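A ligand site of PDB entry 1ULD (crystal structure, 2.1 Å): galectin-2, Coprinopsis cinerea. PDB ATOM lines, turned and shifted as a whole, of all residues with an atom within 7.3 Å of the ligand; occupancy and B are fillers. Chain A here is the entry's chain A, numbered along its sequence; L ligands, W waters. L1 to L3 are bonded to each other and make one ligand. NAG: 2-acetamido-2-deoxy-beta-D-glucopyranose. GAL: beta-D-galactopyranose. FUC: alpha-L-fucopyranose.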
ATOM      1  N   THR A  36      14.812  -2.920 -31.710  1.00  0.00           N
ATOM      2  CA  THR A  36      13.589  -3.592 -31.289  1.00  0.00           C
ATOM      3  C   THR A  36      13.276  -4.758 -32.234  1.00  0.00           C
ATOM      4  O   THR A  36      13.243  -4.595 -33.457  1.00  0.00           O
ATOM      5  CB  THR A  36      12.428  -2.578 -31.248  1.00  0.00           C
ATOM      6  OG1 THR A  36      12.602  -1.715 -30.109  1.00  0.00           O
ATOM      7  CG2 THR A  36      11.081  -3.281 -31.153  1.00  0.00           C
ATOM      8  N   VAL A  38      10.638  -8.114 -32.978  1.00  0.00           N
ATOM      9  CA  VAL A  38       9.325  -8.666 -32.658  1.00  0.00           C
ATOM     10  C   VAL A  38       9.004 -10.032 -33.236  1.00  0.00           C
ATOM     11  O   VAL A  38       9.401 -10.360 -34.349  1.00  0.00           O
ATOM     12  CB  VAL A  38       8.211  -7.678 -33.129  1.00  0.00           C
ATOM     13  CG1 VAL A  38       6.829  -8.315 -32.931  1.00  0.00           C
ATOM     14  CG2 VAL A  38       8.304  -6.363 -32.370  1.00  0.00           C
ATOM     15  N   HIS A  51       2.103 -11.116 -28.934  1.00  0.00           N
ATOM     16  CA  HIS A  51       3.055 -10.155 -29.458  1.00  0.00           C
ATOM     17  C   HIS A  51       4.201 -10.077 -28.458  1.00  0.00           C
ATOM     18  O   HIS A  51       3.972  -9.907 -27.261  1.00  0.00           O
ATOM     19  CB  HIS A  51       2.367  -8.786 -29.552  1.00  0.00           C
ATOM     20  CG  HIS A  51       3.272  -7.661 -29.939  1.00  0.00           C
ATOM     21  ND1 HIS A  51       3.760  -7.495 -31.223  1.00  0.00           N
ATOM     22  CD2 HIS A  51       3.753  -6.616 -29.220  1.00  0.00           C
ATOM     23  CE1 HIS A  51       4.481  -6.393 -31.274  1.00  0.00           C
ATOM     24  NE2 HIS A  51       4.503  -5.840 -30.075  1.00  0.00           N
ATOM     25  N   ILE A  52       5.424 -10.238 -28.936  1.00  0.00           N
ATOM     26  CA  ILE A  52       6.601 -10.175 -28.076  1.00  0.00           C
ATOM     27  C   ILE A  52       7.528  -9.112 -28.664  1.00  0.00           C
ATOM     28  O   ILE A  52       8.167  -9.336 -29.706  1.00  0.00           O
ATOM     29  CB  ILE A  52       7.341 -11.523 -28.012  1.00  0.00           C
ATOM     30  CG1 ILE A  52       6.379 -12.615 -27.552  1.00  0.00           C
ATOM     31  CG2 ILE A  52       8.519 -11.431 -27.036  1.00  0.00           C
ATOM     32  CD1 ILE A  52       6.958 -14.010 -27.600  1.00  0.00           C
ATOM     33  N   SER A  53       7.597  -7.961 -28.005  1.00  0.00           N
ATOM     34  CA  SER A  53       8.412  -6.851 -28.459  1.00  0.00           C
ATOM     35  C   SER A  53       9.652  -6.742 -27.582  1.00  0.00           C
ATOM     36  O   SER A  53       9.586  -6.326 -26.432  1.00  0.00           O
ATOM     37  CB  SER A  53       7.607  -5.543 -28.394  1.00  0.00           C
ATOM     38  OG  SER A  53       8.336  -4.455 -28.944  1.00  0.00           O
ATOM     39  N   ILE A  54      10.792  -7.137 -28.137  1.00  0.00           N
ATOM     40  CA  ILE A  54      12.065  -7.107 -27.416  1.00  0.00           C
ATOM     41  C   ILE A  54      12.690  -5.745 -27.688  1.00  0.00           C
ATOM     42  O   ILE A  54      13.093  -5.449 -28.818  1.00  0.00           O
ATOM     43  CB  ILE A  54      12.959  -8.263 -27.904  1.00  0.00           C
ATOM     44  CG1 ILE A  54      12.178  -9.578 -27.785  1.00  0.00           C
ATOM     45  CG2 ILE A  54      14.241  -8.322 -27.089  1.00  0.00           C
ATOM     46  CD1 ILE A  54      12.780 -10.750 -28.541  1.00  0.00           C
ATOM     47  N   ARG A  55      12.777  -4.917 -26.646  1.00  0.00           N
ATOM     48  CA  ARG A  55      13.305  -3.566 -26.782  1.00  0.00           C
ATOM     49  C   ARG A  55      14.567  -3.320 -25.958  1.00  0.00           C
ATOM     50  O   ARG A  55      14.494  -2.919 -24.785  1.00  0.00           O
ATOM     51  CB  ARG A  55      12.224  -2.556 -26.374  1.00  0.00           C
ATOM     52  CG  ARG A  55      10.859  -2.829 -27.005  1.00  0.00           C
ATOM     53  CD  ARG A  55       9.797  -1.853 -26.507  1.00  0.00           C
ATOM     54  NE  ARG A  55       8.479  -2.122 -27.093  1.00  0.00           N
ATOM     55  CZ  ARG A  55       7.381  -1.441 -26.775  1.00  0.00           C
ATOM     56  NH1 ARG A  55       7.442  -0.449 -25.897  1.00  0.00           N
ATOM     57  NH2 ARG A  55       6.214  -1.750 -27.345  1.00  0.00           N
ATOM     58  N   GLU A  58      15.087   0.249 -24.572  1.00  0.00           N
ATOM     59  CA  GLU A  58      14.175   0.592 -23.491  1.00  0.00           C
ATOM     60  C   GLU A  58      14.393  -0.374 -22.330  1.00  0.00           C
ATOM     61  O   GLU A  58      13.811  -0.209 -21.247  1.00  0.00           O
ATOM     62  CB  GLU A  58      12.740   0.465 -24.013  1.00  0.00           C
ATOM     63  CG  GLU A  58      11.700   1.288 -23.275  1.00  0.00           C
ATOM     64  CD  GLU A  58      10.299   1.025 -23.788  1.00  0.00           C
ATOM     65  OE1 GLU A  58      10.127   0.896 -25.031  1.00  0.00           O
ATOM     66  OE2 GLU A  58       9.362   0.949 -22.956  1.00  0.00           O
ATOM     67  N   VAL A  60      13.405  -3.424 -22.071  1.00  0.00           N
ATOM     68  CA  VAL A  60      12.163  -4.093 -21.724  1.00  0.00           C
ATOM     69  C   VAL A  60      11.706  -5.027 -22.838  1.00  0.00           C
ATOM     70  O   VAL A  60      12.121  -4.901 -23.988  1.00  0.00           O
ATOM     71  CB  VAL A  60      11.032  -3.069 -21.447  1.00  0.00           C
ATOM     72  CG1 VAL A  60      10.579  -2.416 -22.752  1.00  0.00           C
ATOM     73  CG2 VAL A  60       9.874  -3.735 -20.745  1.00  0.00           C
ATOM     74  N   VAL A  62       8.041  -6.373 -24.176  1.00  0.00           N
ATOM     75  CA  VAL A  62       6.605  -6.169 -24.041  1.00  0.00           C
ATOM     76  C   VAL A  62       5.757  -7.263 -24.696  1.00  0.00           C
ATOM     77  O   VAL A  62       6.008  -7.663 -25.835  1.00  0.00           O
ATOM     78  CB  VAL A  62       6.182  -4.813 -24.643  1.00  0.00           C
ATOM     79  CG1 VAL A  62       4.692  -4.551 -24.364  1.00  0.00           C
ATOM     80  CG2 VAL A  62       7.044  -3.688 -24.068  1.00  0.00           C
ATOM     81  N   PHE A  63       4.762  -7.737 -23.945  1.00  0.00           N
ATOM     82  CA  PHE A  63       3.845  -8.759 -24.426  1.00  0.00           C
ATOM     83  C   PHE A  63       2.451  -8.119 -24.561  1.00  0.00           C
ATOM     84  O   PHE A  63       2.055  -7.297 -23.737  1.00  0.00           O
ATOM     85  CB  PHE A  63       3.790  -9.922 -23.443  1.00  0.00           C
ATOM     86  CG  PHE A  63       5.123 -10.593 -23.191  1.00  0.00           C
ATOM     87  CD1 PHE A  63       6.016 -10.066 -22.252  1.00  0.00           C
ATOM     88  CD2 PHE A  63       5.494 -11.724 -23.918  1.00  0.00           C
ATOM     89  CE1 PHE A  63       7.252 -10.677 -22.029  1.00  0.00           C
ATOM     90  CE2 PHE A  63       6.729 -12.335 -23.694  1.00  0.00           C
ATOM     91  CZ  PHE A  63       7.610 -11.815 -22.756  1.00  0.00           C
ATOM     92  N   ASN A  64       1.733  -8.483 -25.614  1.00  0.00           N
ATOM     93  CA  ASN A  64       0.394  -7.933 -25.825  1.00  0.00           C
ATOM     94  C   ASN A  64      -0.344  -8.779 -26.860  1.00  0.00           C
ATOM     95  O   ASN A  64       0.155  -9.828 -27.288  1.00  0.00           O
ATOM     96  CB  ASN A  64       0.493  -6.484 -26.304  1.00  0.00           C
ATOM     97  CG  ASN A  64      -0.652  -5.605 -25.784  1.00  0.00           C
ATOM     98  OD1 ASN A  64      -1.772  -6.087 -25.573  1.00  0.00           O
ATOM     99  ND2 ASN A  64      -0.383  -4.318 -25.601  1.00  0.00           N
ATOM    100  N   SER A  65      -1.533  -8.318 -27.237  1.00  0.00           N
ATOM    101  CA  SER A  65      -2.367  -9.000 -28.232  1.00  0.00           C
ATOM    102  C   SER A  65      -3.297  -7.968 -28.858  1.00  0.00           C
ATOM    103  O   SER A  65      -3.400  -6.833 -28.373  1.00  0.00           O
ATOM    104  CB  SER A  65      -3.219 -10.083 -27.579  1.00  0.00           C
ATOM    105  OG  SER A  65      -2.454 -10.861 -26.674  1.00  0.00           O
ATOM    106  N   ARG A  66      -3.980  -8.353 -29.932  1.00  0.00           N
ATOM    107  CA  ARG A  66      -4.925  -7.474 -30.611  1.00  0.00           C
ATOM    108  C   ARG A  66      -5.454  -8.145 -31.866  1.00  0.00           C
ATOM    109  O   ARG A  66      -4.753  -8.920 -32.520  1.00  0.00           O
ATOM    110  CB  ARG A  66      -4.256  -6.151 -30.991  1.00  0.00           C
ATOM    111  CG  ARG A  66      -3.363  -6.210 -32.226  1.00  0.00           C
ATOM    112  CD  ARG A  66      -2.703  -4.866 -32.437  1.00  0.00           C
ATOM    113  NE  ARG A  66      -1.991  -4.757 -33.709  1.00  0.00           N
ATOM    114  CZ  ARG A  66      -2.567  -4.778 -34.902  1.00  0.00           C
ATOM    115  NH1 ARG A  66      -3.887  -4.913 -35.014  1.00  0.00           N
ATOM    116  NH2 ARG A  66      -1.824  -4.677 -36.003  1.00  0.00           N
ATOM    117  N   TRP A  72      -4.346  -2.695 -29.251  1.00  0.00           N
ATOM    118  CA  TRP A  72      -3.557  -3.428 -28.264  1.00  0.00           C
ATOM    119  C   TRP A  72      -4.315  -3.319 -26.951  1.00  0.00           C
ATOM    120  O   TRP A  72      -5.075  -2.386 -26.750  1.00  0.00           O
ATOM    121  CB  TRP A  72      -2.171  -2.788 -28.062  1.00  0.00           C
ATOM    122  CG  TRP A  72      -1.260  -2.851 -29.258  1.00  0.00           C
ATOM    123  CD1 TRP A  72      -0.822  -1.794 -30.006  1.00  0.00           C
ATOM    124  CD2 TRP A  72      -0.659  -4.017 -29.816  1.00  0.00           C
ATOM    125  NE1 TRP A  72       0.005  -2.232 -31.001  1.00  0.00           N
ATOM    126  CE2 TRP A  72       0.133  -3.592 -30.914  1.00  0.00           C
ATOM    127  CE3 TRP A  72      -0.710  -5.382 -29.503  1.00  0.00           C
ATOM    128  CZ2 TRP A  72       0.863  -4.496 -31.697  1.00  0.00           C
ATOM    129  CZ3 TRP A  72       0.020  -6.273 -30.285  1.00  0.00           C
ATOM    130  CH2 TRP A  72       0.797  -5.820 -31.369  1.00  0.00           C
ATOM    131  N   GLY A  73      -4.108  -4.286 -26.068  1.00  0.00           N
ATOM    132  CA  GLY A  73      -4.758  -4.242 -24.779  1.00  0.00           C
ATOM    133  C   GLY A  73      -3.713  -3.713 -23.823  1.00  0.00           C
ATOM    134  O   GLY A  73      -2.796  -3.011 -24.248  1.00  0.00           O
ATOM    135  N   PRO A  74      -3.831  -3.997 -22.519  1.00  0.00           N
ATOM    136  CA  PRO A  74      -2.793  -3.486 -21.621  1.00  0.00           C
ATOM    137  C   PRO A  74      -1.507  -4.260 -21.876  1.00  0.00           C
ATOM    138  O   PRO A  74      -1.546  -5.414 -22.316  1.00  0.00           O
ATOM    139  CB  PRO A  74      -3.373  -3.747 -20.229  1.00  0.00           C
ATOM    140  CG  PRO A  74      -4.238  -4.959 -20.449  1.00  0.00           C
ATOM    141  CD  PRO A  74      -4.916  -4.646 -21.755  1.00  0.00           C
ATOM    142  N   GLU A  75      -0.365  -3.631 -21.630  1.00  0.00           N
ATOM    143  CA  GLU A  75       0.909  -4.293 -21.850  1.00  0.00           C
ATOM    144  C   GLU A  75       1.372  -5.056 -20.632  1.00  0.00           C
ATOM    145  O   GLU A  75       1.029  -4.723 -19.498  1.00  0.00           O
ATOM    146  CB  GLU A  75       2.004  -3.280 -22.204  1.00  0.00           C
ATOM    147  CG  GLU A  75       1.717  -2.410 -23.389  1.00  0.00           C
ATOM    148  CD  GLU A  75       2.896  -1.521 -23.717  1.00  0.00           C
ATOM    149  OE1 GLU A  75       3.611  -1.125 -22.766  1.00  0.00           O
ATOM    150  OE2 GLU A  75       3.105  -1.211 -24.902  1.00  0.00           O
ATOM    151  N   GLU A  76       2.161  -6.086 -20.879  1.00  0.00           N
ATOM    152  CA  GLU A  76       2.739  -6.874 -19.805  1.00  0.00           C
ATOM    153  C   GLU A  76       4.232  -6.815 -20.126  1.00  0.00           C
ATOM    154  O   GLU A  76       4.661  -7.159 -21.229  1.00  0.00           O
ATOM    155  CB  GLU A  76       2.168  -8.281 -19.808  1.00  0.00           C
ATOM    156  CG  GLU A  76       0.701  -8.267 -19.386  1.00  0.00           C
ATOM    157  CD  GLU A  76       0.106  -9.641 -19.191  1.00  0.00           C
ATOM    158  OE1 GLU A  76       0.696 -10.443 -18.430  1.00  0.00           O
ATOM    159  OE2 GLU A  76      -0.952  -9.916 -19.799  1.00  0.00           O
ATOM    160  N   ARG A  77       5.007  -6.351 -19.146  1.00  0.00           N
ATOM    161  CA  ARG A  77       6.439  -6.162 -19.331  1.00  0.00           C
ATOM    162  C   ARG A  77       7.352  -6.871 -18.330  1.00  0.00           C
ATOM    163  O   ARG A  77       6.928  -7.263 -17.245  1.00  0.00           O
ATOM    164  CB  ARG A  77       6.746  -4.666 -19.261  1.00  0.00           C
ATOM    165  CG  ARG A  77       5.910  -3.785 -20.193  1.00  0.00           C
ATOM    166  CD  ARG A  77       6.195  -2.304 -19.938  1.00  0.00           C
ATOM    167  NE  ARG A  77       5.891  -1.490 -21.114  1.00  0.00           N
ATOM    168  CZ  ARG A  77       6.697  -0.556 -21.599  1.00  0.00           C
ATOM    169  NH1 ARG A  77       7.871  -0.303 -21.020  1.00  0.00           N
ATOM    170  NH2 ARG A  77       6.343   0.099 -22.694  1.00  0.00           N
HETATM  171  C1  NAG L   1       3.311   3.916 -25.322  1.00  0.00           C
HETATM  172  C2  NAG L   1       3.687   2.541 -24.748  1.00  0.00           C
HETATM  173  C3  NAG L   1       4.479   1.782 -25.810  1.00  0.00           C
HETATM  174  C4  NAG L   1       3.644   1.672 -27.078  1.00  0.00           C
HETATM  175  C5  NAG L   1       3.215   3.073 -27.556  1.00  0.00           C
HETATM  176  C6  NAG L   1       2.295   3.048 -28.771  1.00  0.00           C
HETATM  177  C7  NAG L   1       3.893   2.397 -22.362  1.00  0.00           C
HETATM  178  C8  NAG L   1       4.804   2.351 -21.145  1.00  0.00           C
HETATM  179  N2  NAG L   1       4.454   2.683 -23.533  1.00  0.00           N
HETATM  180  O1  NAG L   1       2.566   4.615 -24.381  1.00  0.00           O
HETATM  181  O3  NAG L   1       4.803   0.483 -25.334  1.00  0.00           O
HETATM  182  O4  NAG L   1       4.391   1.026 -28.115  1.00  0.00           O
HETATM  183  O5  NAG L   1       2.512   3.758 -26.496  1.00  0.00           O
HETATM  184  O6  NAG L   1       1.160   2.240 -28.533  1.00  0.00           O
HETATM  185  O7  NAG L   1       2.691   2.183 -22.239  1.00  0.00           O
HETATM  186  C1  GAL L   2       3.707   0.074 -28.851  1.00  0.00           C
HETATM  187  C2  GAL L   2       4.535  -0.311 -30.075  1.00  0.00           C
HETATM  188  C3  GAL L   2       3.903  -1.491 -30.812  1.00  0.00           C
HETATM  189  C4  GAL L   2       3.650  -2.648 -29.839  1.00  0.00           C
HETATM  190  C5  GAL L   2       2.790  -2.132 -28.688  1.00  0.00           C
HETATM  191  C6  GAL L   2       2.477  -3.204 -27.662  1.00  0.00           C
HETATM  192  O2  GAL L   2       4.630   0.812 -30.975  1.00  0.00           O
HETATM  193  O3  GAL L   2       4.765  -1.920 -31.861  1.00  0.00           O
HETATM  194  O4  GAL L   2       4.897  -3.123 -29.337  1.00  0.00           O
HETATM  195  O5  GAL L   2       3.471  -1.056 -28.004  1.00  0.00           O
HETATM  196  O6  GAL L   2       1.658  -2.692 -26.622  1.00  0.00           O
HETATM  197  C1  FUC L   3       5.883   1.023 -31.557  1.00  0.00           C
HETATM  198  C2  FUC L   3       5.788   2.137 -32.606  1.00  0.00           C
HETATM  199  C3  FUC L   3       5.474   3.458 -31.901  1.00  0.00           C
HETATM  200  C4  FUC L   3       6.543   3.755 -30.835  1.00  0.00           C
HETATM  201  C5  FUC L   3       6.673   2.574 -29.872  1.00  0.00           C
HETATM  202  C6  FUC L   3       7.852   2.738 -28.927  1.00  0.00           C
HETATM  203  O2  FUC L   3       4.774   1.832 -33.535  1.00  0.00           O
HETATM  204  O3  FUC L   3       5.458   4.502 -32.863  1.00  0.00           O
HETATM  205  O4  FUC L   3       7.794   3.997 -31.468  1.00  0.00           O
HETATM  206  O5  FUC L   3       6.895   1.348 -30.598  1.00  0.00           O
HETATM  207  O   HOH W   1       2.016   6.872 -22.628  1.00  0.00           O
HETATM  208  O   HOH W   2       3.817  -3.083 -33.863  1.00  0.00           O
HETATM  209  O   HOH W   3       8.546  -0.832 -29.915  1.00  0.00           O
HETATM  210  O   HOH W   4       0.626   0.790 -23.809  1.00  0.00           O
HETATM  211  O   HOH W   5       7.274   2.761 -24.311  1.00  0.00           O
HETATM  212  O   HOH W   6       7.434  -3.066 -31.024  1.00  0.00           O
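The side-chain carboxylate of Glu 75 is in hydrogen-bond range of an oxygen (O3) of NAG L1, at 2.4 Å.
O4 of GAL L2 lies within hydrogen-bond range of NH2 of Arg 55 (2.8 Å).
An oxygen (O6) of GAL L2 is in hydrogen-bond range of the side-chain amide nitrogen (ND2) of Asn 64 (2.8 Å).
NE2 of His 51 sits at hydrogen-bond distance from O4 of GAL L2 (2.8 Å).
The guanidinium group (NH2) of Arg 77 lies within hydrogen-bond range of an oxygen (O3) of NAG L1, at 3.1 Å.
The side-chain carboxylate (OE2) of Glu 75 is in salt-bridge range of the guanidinium group (NH2) of Arg 55 (3.99 Å).
The guanidinium group of Arg 77 is in salt-bridge range of the side-chain carboxylate of Glu 75, 2.8 Å away.
The guanidinium group (NE) of Arg 55 sits at hydrogen-bond distance from the side-chain hydroxyl (OG) of Ser 53.
OE1 of Glu 58 lies within salt-bridge range of NH1 of Arg 55, 3.1 Å away.
The backbone carbonyl oxygen of Val 60 lies within hydrogen-bond range of the backbone NH of Arg 55 (2.7 Å).
The backbone carbonyl oxygen of Asn 64 sits at hydrogen-bond distance from the backbone NH of His 51, 2.9 Å away.
OD1 of Asn 64 is in hydrogen-bond range of N of Gly 73, at 3.0 Å.
O of Pro 74 sits close to OD1 of Asn 64.
Ser 53 touches the ligand.
Trp 72 touches the ligand.
Within 4 Å of the ligand: His 51, Ser 53, Arg 55, Asn 64, Trp 72, Glu 75 and Arg 77.
Water W3 lies within hydrogen-bond range of O5 of FUC L3 (2.8 Å) and NE of Arg 55 (3.1 Å).
Water W5 lies within hydrogen-bond range of N2 of NAG L1, OE2 of Glu 58 and NH2 of Arg 77.
Water W4 bridges an oxygen (O7) of NAG L1 (2.9 Å) and the side-chain carboxylate (OE2) of Glu 75 (3.4 Å).
Water W6 bridges OG of Ser 53 (2.7 Å) and O3 of GAL L2 (3.0 Å).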
